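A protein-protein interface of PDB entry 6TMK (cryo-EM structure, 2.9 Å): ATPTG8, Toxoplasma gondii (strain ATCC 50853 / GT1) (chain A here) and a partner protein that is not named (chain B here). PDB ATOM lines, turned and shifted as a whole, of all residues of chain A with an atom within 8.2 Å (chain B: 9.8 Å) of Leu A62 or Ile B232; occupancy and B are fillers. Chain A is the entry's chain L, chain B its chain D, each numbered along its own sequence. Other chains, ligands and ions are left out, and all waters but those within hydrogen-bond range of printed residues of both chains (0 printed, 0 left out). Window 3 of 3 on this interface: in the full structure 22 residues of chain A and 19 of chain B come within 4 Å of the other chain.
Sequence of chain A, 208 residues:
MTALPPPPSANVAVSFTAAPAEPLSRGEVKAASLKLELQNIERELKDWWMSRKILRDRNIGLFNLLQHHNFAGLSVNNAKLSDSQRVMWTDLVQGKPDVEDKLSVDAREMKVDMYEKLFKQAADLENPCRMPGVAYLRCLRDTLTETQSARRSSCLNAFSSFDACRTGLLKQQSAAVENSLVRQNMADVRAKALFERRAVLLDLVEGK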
ATOM      1  N   LEU A  55     -23.334  12.196  22.473  1.00  0.00           N
ATOM      2  CA  LEU A  55     -22.357  11.516  23.312  1.00  0.00           C
ATOM      3  C   LEU A  55     -21.283  10.836  22.478  1.00  0.00           C
ATOM      4  O   LEU A  55     -20.096  10.897  22.819  1.00  0.00           O
ATOM      5  CB  LEU A  55     -23.063  10.514  24.215  1.00  0.00           C
ATOM      6  CG  LEU A  55     -23.682  11.126  25.462  1.00  0.00           C
ATOM      7  CD1 LEU A  55     -24.629  10.158  26.097  1.00  0.00           C
ATOM      8  CD2 LEU A  55     -22.618  11.535  26.446  1.00  0.00           C
ATOM      9  N   ARG A  56     -21.671  10.188  21.380  1.00  0.00           N
ATOM     10  CA  ARG A  56     -20.688   9.577  20.495  1.00  0.00           C
ATOM     11  C   ARG A  56     -19.694  10.609  19.992  1.00  0.00           C
ATOM     12  O   ARG A  56     -18.476  10.398  20.046  1.00  0.00           O
ATOM     13  CB  ARG A  56     -21.396   8.898  19.332  1.00  0.00           C
ATOM     14  CG  ARG A  56     -20.573   7.855  18.628  1.00  0.00           C
ATOM     15  CD  ARG A  56     -21.288   7.334  17.417  1.00  0.00           C
ATOM     16  NE  ARG A  56     -20.378   7.042  16.319  1.00  0.00           N
ATOM     17  CZ  ARG A  56     -19.522   6.032  16.315  1.00  0.00           C
ATOM     18  NH1 ARG A  56     -19.455   5.214  17.351  1.00  0.00           N
ATOM     19  NH2 ARG A  56     -18.735   5.843  15.273  1.00  0.00           N
ATOM     20  N   ASP A  57     -20.197  11.740  19.498  1.00  0.00           N
ATOM     21  CA  ASP A  57     -19.315  12.766  18.956  1.00  0.00           C
ATOM     22  C   ASP A  57     -18.387  13.316  20.031  1.00  0.00           C
ATOM     23  O   ASP A  57     -17.177  13.454  19.813  1.00  0.00           O
ATOM     24  CB  ASP A  57     -20.142  13.880  18.324  1.00  0.00           C
ATOM     25  CG  ASP A  57     -20.793  13.455  17.022  1.00  0.00           C
ATOM     26  OD1 ASP A  57     -21.529  14.270  16.429  1.00  0.00           O
ATOM     27  OD2 ASP A  57     -20.564  12.307  16.586  1.00  0.00           O
ATOM     28  N   ARG A  58     -18.933  13.628  21.206  1.00  0.00           N
ATOM     29  CA  ARG A  58     -18.116  14.178  22.279  1.00  0.00           C
ATOM     30  C   ARG A  58     -17.018  13.207  22.681  1.00  0.00           C
ATOM     31  O   ARG A  58     -15.862  13.603  22.866  1.00  0.00           O
ATOM     32  CB  ARG A  58     -18.988  14.513  23.484  1.00  0.00           C
ATOM     33  CG  ARG A  58     -18.197  14.889  24.713  1.00  0.00           C
ATOM     34  CD  ARG A  58     -19.064  15.395  25.820  1.00  0.00           C
ATOM     35  NE  ARG A  58     -18.288  15.626  27.029  1.00  0.00           N
ATOM     36  CZ  ARG A  58     -17.551  16.706  27.248  1.00  0.00           C
ATOM     37  NH1 ARG A  58     -17.488  17.665  26.349  1.00  0.00           N
ATOM     38  NH2 ARG A  58     -16.872  16.826  28.369  1.00  0.00           N
ATOM     39  N   ASN A  59     -17.359  11.931  22.840  1.00  0.00           N
ATOM     40  CA  ASN A  59     -16.380  10.990  23.357  1.00  0.00           C
ATOM     41  C   ASN A  59     -15.336  10.638  22.309  1.00  0.00           C
ATOM     42  O   ASN A  59     -14.170  10.417  22.652  1.00  0.00           O
ATOM     43  CB  ASN A  59     -17.094   9.744  23.861  1.00  0.00           C
ATOM     44  CG  ASN A  59     -17.978  10.035  25.046  1.00  0.00           C
ATOM     45  OD1 ASN A  59     -19.184   9.818  25.007  1.00  0.00           O
ATOM     46  ND2 ASN A  59     -17.387  10.558  26.099  1.00  0.00           N
ATOM     47  N   ILE A  60     -15.709  10.625  21.031  1.00  0.00           N
ATOM     48  CA  ILE A  60     -14.702  10.451  19.992  1.00  0.00           C
ATOM     49  C   ILE A  60     -13.771  11.654  19.952  1.00  0.00           C
ATOM     50  O   ILE A  60     -12.559  11.510  19.748  1.00  0.00           O
ATOM     51  CB  ILE A  60     -15.366  10.187  18.633  1.00  0.00           C
ATOM     52  CG1 ILE A  60     -15.828   8.737  18.556  1.00  0.00           C
ATOM     53  CG2 ILE A  60     -14.409  10.468  17.514  1.00  0.00           C
ATOM     54  CD1 ILE A  60     -16.921   8.499  17.598  1.00  0.00           C
ATOM     55  N   GLY A  61     -14.311  12.855  20.149  1.00  0.00           N
ATOM     56  CA  GLY A  61     -13.457  14.026  20.206  1.00  0.00           C
ATOM     57  C   GLY A  61     -12.489  13.984  21.370  1.00  0.00           C
ATOM     58  O   GLY A  61     -11.319  14.341  21.229  1.00  0.00           O
ATOM     59  N   LEU A  62     -12.965  13.557  22.540  1.00  0.00           N
ATOM     60  CA  LEU A  62     -12.073  13.385  23.683  1.00  0.00           C
ATOM     61  C   LEU A  62     -10.987  12.363  23.391  1.00  0.00           C
ATOM     62  O   LEU A  62      -9.819  12.571  23.731  1.00  0.00           O
ATOM     63  CB  LEU A  62     -12.850  12.979  24.929  1.00  0.00           C
ATOM     64  CG  LEU A  62     -13.722  14.014  25.609  1.00  0.00           C
ATOM     65  CD1 LEU A  62     -14.532  13.374  26.687  1.00  0.00           C
ATOM     66  CD2 LEU A  62     -12.813  15.044  26.213  1.00  0.00           C
ATOM     67  N   PHE A  63     -11.358  11.230  22.801  1.00  0.00           N
ATOM     68  CA  PHE A  63     -10.358  10.224  22.478  1.00  0.00           C
ATOM     69  C   PHE A  63      -9.305  10.784  21.539  1.00  0.00           C
ATOM     70  O   PHE A  63      -8.106  10.563  21.737  1.00  0.00           O
ATOM     71  CB  PHE A  63     -11.019   9.004  21.854  1.00  0.00           C
ATOM     72  CG  PHE A  63     -10.044   8.025  21.285  1.00  0.00           C
ATOM     73  CD1 PHE A  63      -9.329   7.188  22.114  1.00  0.00           C
ATOM     74  CD2 PHE A  63      -9.826   7.955  19.929  1.00  0.00           C
ATOM     75  CE1 PHE A  63      -8.433   6.297  21.601  1.00  0.00           C
ATOM     76  CE2 PHE A  63      -8.929   7.062  19.413  1.00  0.00           C
ATOM     77  CZ  PHE A  63      -8.229   6.235  20.250  1.00  0.00           C
ATOM     78  N   ASN A  64      -9.731  11.513  20.511  1.00  0.00           N
ATOM     79  CA  ASN A  64      -8.772  12.064  19.562  1.00  0.00           C
ATOM     80  C   ASN A  64      -7.891  13.112  20.220  1.00  0.00           C
ATOM     81  O   ASN A  64      -6.695  13.193  19.929  1.00  0.00           O
ATOM     82  CB  ASN A  64      -9.513  12.658  18.372  1.00  0.00           C
ATOM     83  CG  ASN A  64     -10.004  11.604  17.414  1.00  0.00           C
ATOM     84  OD1 ASN A  64      -9.375  10.565  17.232  1.00  0.00           O
ATOM     85  ND2 ASN A  64     -11.138  11.867  16.796  1.00  0.00           N
ATOM     86  N   LEU A  65      -8.454  13.899  21.132  1.00  0.00           N
ATOM     87  CA  LEU A  65      -7.662  14.886  21.852  1.00  0.00           C
ATOM     88  C   LEU A  65      -6.613  14.223  22.736  1.00  0.00           C
ATOM     89  O   LEU A  65      -5.458  14.664  22.786  1.00  0.00           O
ATOM     90  CB  LEU A  65      -8.592  15.758  22.685  1.00  0.00           C
ATOM     91  CG  LEU A  65      -7.977  16.830  23.566  1.00  0.00           C
ATOM     92  CD1 LEU A  65      -7.350  17.875  22.701  1.00  0.00           C
ATOM     93  CD2 LEU A  65      -9.027  17.432  24.455  1.00  0.00           C
ATOM     94  N   LEU A  66      -7.005  13.178  23.463  1.00  0.00           N
ATOM     95  CA  LEU A  66      -6.067  12.486  24.336  1.00  0.00           C
ATOM     96  C   LEU A  66      -4.989  11.769  23.536  1.00  0.00           C
ATOM     97  O   LEU A  66      -3.825  11.735  23.944  1.00  0.00           O
ATOM     98  CB  LEU A  66      -6.819  11.495  25.220  1.00  0.00           C
ATOM     99  CG  LEU A  66      -7.895  12.077  26.126  1.00  0.00           C
ATOM    100  CD1 LEU A  66      -8.854  10.995  26.557  1.00  0.00           C
ATOM    101  CD2 LEU A  66      -7.284  12.740  27.325  1.00  0.00           C
ATOM    102  N   GLN A  67      -5.357  11.197  22.391  1.00  0.00           N
ATOM    103  CA  GLN A  67      -4.372  10.593  21.506  1.00  0.00           C
ATOM    104  C   GLN A  67      -3.429  11.647  20.943  1.00  0.00           C
ATOM    105  O   GLN A  67      -2.238  11.389  20.746  1.00  0.00           O
ATOM    106  CB  GLN A  67      -5.089   9.842  20.387  1.00  0.00           C
ATOM    107  CG  GLN A  67      -4.404   8.589  19.915  1.00  0.00           C
ATOM    108  CD  GLN A  67      -5.089   7.979  18.718  1.00  0.00           C
ATOM    109  OE1 GLN A  67      -5.674   8.685  17.898  1.00  0.00           O
ATOM    110  NE2 GLN A  67      -5.019   6.659  18.605  1.00  0.00           N
ATOM    111  N   HIS A  68      -3.954  12.843  20.687  1.00  0.00           N
ATOM    112  CA  HIS A  68      -3.148  13.935  20.163  1.00  0.00           C
ATOM    113  C   HIS A  68      -2.122  14.400  21.183  1.00  0.00           C
ATOM    114  O   HIS A  68      -0.958  14.632  20.842  1.00  0.00           O
ATOM    115  CB  HIS A  68      -4.090  15.074  19.776  1.00  0.00           C
ATOM    116  CG  HIS A  68      -3.422  16.260  19.165  1.00  0.00           C
ATOM    117  ND1 HIS A  68      -3.602  17.536  19.651  1.00  0.00           N
ATOM    118  CD2 HIS A  68      -2.620  16.379  18.083  1.00  0.00           C
ATOM    119  CE1 HIS A  68      -2.917  18.386  18.910  1.00  0.00           C
ATOM    120  NE2 HIS A  68      -2.311  17.709  17.952  1.00  0.00           N
ATOM    121  N   HIS A  69      -2.540  14.560  22.432  1.00  0.00           N
ATOM    122  CA  HIS A  69      -1.650  14.977  23.503  1.00  0.00           C
ATOM    123  C   HIS A  69      -0.923  13.814  24.171  1.00  0.00           C
ATOM    124  O   HIS A  69      -0.216  14.028  25.159  1.00  0.00           O
ATOM    125  CB  HIS A  69      -2.433  15.779  24.536  1.00  0.00           C
ATOM    126  CG  HIS A  69      -2.861  17.123  24.042  1.00  0.00           C
ATOM    127  ND1 HIS A  69      -1.985  18.017  23.472  1.00  0.00           N
ATOM    128  CD2 HIS A  69      -4.077  17.712  24.006  1.00  0.00           C
ATOM    129  CE1 HIS A  69      -2.642  19.107  23.119  1.00  0.00           C
ATOM    130  NE2 HIS A  69      -3.912  18.947  23.432  1.00  0.00           N
ATOM    131  N   PHE A  71      -1.729  10.807  25.912  1.00  0.00           N
ATOM    132  CA  PHE A  71      -2.097  10.446  27.270  1.00  0.00           C
ATOM    133  C   PHE A  71      -2.120   8.937  27.449  1.00  0.00           C
ATOM    134  O   PHE A  71      -2.315   8.178  26.497  1.00  0.00           O
ATOM    135  CB  PHE A  71      -3.460  11.017  27.653  1.00  0.00           C
ATOM    136  CG  PHE A  71      -3.411  12.413  28.177  1.00  0.00           C
ATOM    137  CD1 PHE A  71      -3.426  12.642  29.537  1.00  0.00           C
ATOM    138  CD2 PHE A  71      -3.331  13.490  27.327  1.00  0.00           C
ATOM    139  CE1 PHE A  71      -3.379  13.911  30.033  1.00  0.00           C
ATOM    140  CE2 PHE A  71      -3.281  14.765  27.821  1.00  0.00           C
ATOM    141  CZ  PHE A  71      -3.302  14.978  29.175  1.00  0.00           C
ATOM    142  N   ARG B 178     -21.625  28.529  18.196  1.00  0.00           N
ATOM    143  CA  ARG B 178     -21.283  27.127  17.987  1.00  0.00           C
ATOM    144  C   ARG B 178     -22.423  26.217  18.420  1.00  0.00           C
ATOM    145  O   ARG B 178     -22.777  25.261  17.718  1.00  0.00           O
ATOM    146  CB  ARG B 178     -20.021  26.779  18.754  1.00  0.00           C
ATOM    147  CG  ARG B 178     -18.767  27.270  18.147  1.00  0.00           C
ATOM    148  CD  ARG B 178     -17.621  26.492  18.697  1.00  0.00           C
ATOM    149  NE  ARG B 178     -17.490  26.683  20.137  1.00  0.00           N
ATOM    150  CZ  ARG B 178     -16.780  27.654  20.704  1.00  0.00           C
ATOM    151  NH1 ARG B 178     -16.134  28.541  19.963  1.00  0.00           N
ATOM    152  NH2 ARG B 178     -16.726  27.736  22.021  1.00  0.00           N
ATOM    153  N   HIS B 182     -24.443  23.676  15.848  1.00  0.00           N
ATOM    154  CA  HIS B 182     -24.440  22.247  16.124  1.00  0.00           C
ATOM    155  C   HIS B 182     -25.861  21.720  16.296  1.00  0.00           C
ATOM    156  O   HIS B 182     -26.221  20.671  15.747  1.00  0.00           O
ATOM    157  CB  HIS B 182     -23.597  21.987  17.368  1.00  0.00           C
ATOM    158  CG  HIS B 182     -23.191  20.563  17.551  1.00  0.00           C
ATOM    159  ND1 HIS B 182     -22.625  20.103  18.720  1.00  0.00           N
ATOM    160  CD2 HIS B 182     -23.257  19.498  16.721  1.00  0.00           C
ATOM    161  CE1 HIS B 182     -22.368  18.815  18.603  1.00  0.00           C
ATOM    162  NE2 HIS B 182     -22.742  18.423  17.400  1.00  0.00           N
ATOM    163  N   GLN B 229     -16.003  16.078  15.106  1.00  0.00           N
ATOM    164  CA  GLN B 229     -15.339  15.130  15.993  1.00  0.00           C
ATOM    165  C   GLN B 229     -13.846  15.399  16.093  1.00  0.00           C
ATOM    166  O   GLN B 229     -13.074  14.498  16.411  1.00  0.00           O
ATOM    167  CB  GLN B 229     -15.559  13.698  15.517  1.00  0.00           C
ATOM    168  CG  GLN B 229     -17.006  13.266  15.462  1.00  0.00           C
ATOM    169  CD  GLN B 229     -17.169  11.878  14.880  1.00  0.00           C
ATOM    170  OE1 GLN B 229     -16.358  11.437  14.068  1.00  0.00           O
ATOM    171  NE2 GLN B 229     -18.215  11.176  15.301  1.00  0.00           N
ATOM    172  N   ASN B 230     -13.434  16.637  15.821  1.00  0.00           N
ATOM    173  CA  ASN B 230     -12.010  16.951  15.859  1.00  0.00           C
ATOM    174  C   ASN B 230     -11.489  16.857  17.285  1.00  0.00           C
ATOM    175  O   ASN B 230     -10.662  15.996  17.605  1.00  0.00           O
ATOM    176  CB  ASN B 230     -11.776  18.345  15.280  1.00  0.00           C
ATOM    177  CG  ASN B 230     -10.353  18.559  14.831  1.00  0.00           C
ATOM    178  OD1 ASN B 230      -9.657  17.615  14.462  1.00  0.00           O
ATOM    179  ND2 ASN B 230      -9.912  19.811  14.851  1.00  0.00           N
ATOM    180  N   GLY B 231     -11.981  17.722  18.161  1.00  0.00           N
ATOM    181  CA  GLY B 231     -11.724  17.592  19.576  1.00  0.00           C
ATOM    182  C   GLY B 231     -12.996  17.875  20.340  1.00  0.00           C
ATOM    183  O   GLY B 231     -14.043  17.289  20.057  1.00  0.00           O
ATOM    184  N   ILE B 232     -12.920  18.781  21.304  1.00  0.00           N
ATOM    185  CA  ILE B 232     -14.108  19.269  21.990  1.00  0.00           C
ATOM    186  C   ILE B 232     -14.056  20.789  22.040  1.00  0.00           C
ATOM    187  O   ILE B 232     -13.005  21.385  21.770  1.00  0.00           O
ATOM    188  CB  ILE B 232     -14.242  18.673  23.397  1.00  0.00           C
ATOM    189  CG1 ILE B 232     -12.994  18.952  24.218  1.00  0.00           C
ATOM    190  CG2 ILE B 232     -14.496  17.195  23.317  1.00  0.00           C
ATOM    191  CD1 ILE B 232     -13.215  18.826  25.666  1.00  0.00           C
ATOM    192  N   PRO B 233     -15.159  21.453  22.380  1.00  0.00           N
ATOM    193  CA  PRO B 233     -15.078  22.867  22.703  1.00  0.00           C
ATOM    194  C   PRO B 233     -14.372  23.068  24.029  1.00  0.00           C
ATOM    195  O   PRO B 233     -14.370  22.171  24.887  1.00  0.00           O
ATOM    196  CB  PRO B 233     -16.553  23.299  22.779  1.00  0.00           C
ATOM    197  CG  PRO B 233     -17.296  22.264  22.088  1.00  0.00           C
ATOM    198  CD  PRO B 233     -16.546  21.006  22.206  1.00  0.00           C
ATOM    199  N   PRO B 234     -13.763  24.225  24.246  1.00  0.00           N
ATOM    200  CA  PRO B 234     -13.108  24.468  25.530  1.00  0.00           C
ATOM    201  C   PRO B 234     -14.111  24.534  26.665  1.00  0.00           C
ATOM    202  O   PRO B 234     -15.250  24.981  26.507  1.00  0.00           O
ATOM    203  CB  PRO B 234     -12.401  25.808  25.326  1.00  0.00           C
ATOM    204  CG  PRO B 234     -12.297  25.967  23.880  1.00  0.00           C
ATOM    205  CD  PRO B 234     -13.451  25.280  23.273  1.00  0.00           C
ATOM    206  N   SER B 235     -13.657  24.088  27.831  1.00  0.00           N
ATOM    207  CA  SER B 235     -14.498  24.091  29.017  1.00  0.00           C
ATOM    208  C   SER B 235     -14.520  25.462  29.672  1.00  0.00           C
ATOM    209  O   SER B 235     -15.563  25.900  30.170  1.00  0.00           O
ATOM    210  CB  SER B 235     -13.986  23.035  29.990  1.00  0.00           C
ATOM    211  OG  SER B 235     -13.717  21.825  29.311  1.00  0.00           O
ATOM    212  N   VAL B 236     -13.380  26.147  29.685  1.00  0.00           N
ATOM    213  CA  VAL B 236     -13.258  27.460  30.293  1.00  0.00           C
ATOM    214  C   VAL B 236     -12.398  28.330  29.391  1.00  0.00           C
ATOM    215  O   VAL B 236     -11.642  27.840  28.551  1.00  0.00           O
ATOM    216  CB  VAL B 236     -12.665  27.396  31.715  1.00  0.00           C
ATOM    217  CG1 VAL B 236     -13.662  26.782  32.660  1.00  0.00           C
ATOM    218  CG2 VAL B 236     -11.394  26.599  31.722  1.00  0.00           C
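The side-chain amide nitrogen of Gln B229 lies within hydrogen-bond range of the side-chain carboxylate of Asp A57, 2.9 Å away.
O of Gln B229 is in hydrogen-bond range of ND2 of Asn A64 (3.3 Å).
The backbone carbonyl oxygen of Ile A60 lies within hydrogen-bond range of the side-chain amide nitrogen of Asn A64 (3.3 Å).
O of Arg A58 touches CG2 of Ile B232, 3.9 Å away.
CD1 of Ile A60 touches NE2 of Gln B229 (3.8 Å).
CA of Gly A61 touches O of Gln B229, at 3.8 Å.
CA of Gly A61 touches O of Gly B231 (3.3 Å).
Ile B232 touches Leu A62.
CB of Asn A64 touches O of Asn B230, at 3.6 Å.
Printed residues of chain B within 4 Å of Asp A57: Gln B229.
Of the printed residues of chain B, Arg A58 touches Ile B232 (3.9 Å).
Printed residues of chain B within 4 Å of Ile A60: Gln B229 (3.8 Å).
Gly A61 touches just these residues of chain B: Gln B229 (3.8 Å) and Gly B231 (3.3 Å).
Leu A62 touches one residue of chain B.
Of the printed residues of chain B, Asn A64 touches Gln B229 (3.3 Å) and Asn B230 (3.6 Å).
Of chain A, only Arg A58 (3.9 Å) and Leu A62 (3.8 Å) come within 4 Å of Ile B232.
No residue of chain A comes within 4 Å of Pro B233.
The nearest printed residue of chain A that does not touch Ile B232 is Leu A65 (4.3 Å).
The nearest printed residue of chain B that does not touch Asn A64 is Gly B231 (5.5 Å).
Of the 10 printed residues of chain B, 4 touch a printed residue of chain A.
Printed residues of chain B that touch a printed residue of chain A: Gln B229, Asn B230, Gly B231 and Ile B232.
Hydrophobic or aromatic side chains of chain B that line the printed part of chain A: Ile B232.
Printed residues of chain A that touch a printed residue of chain B: Asp A57, Arg A58, Ile A60, Gly A61, Leu A62 and Asn A64.
Hydrophobic or aromatic side chains of chain A within 4 Å of the printed part of chain B: Ile A60 and Leu A62.
Among the printed residues, no Asp or Glu carboxylate lies within 4 Å of a Lys or Arg side-chain nitrogen of the other chain.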
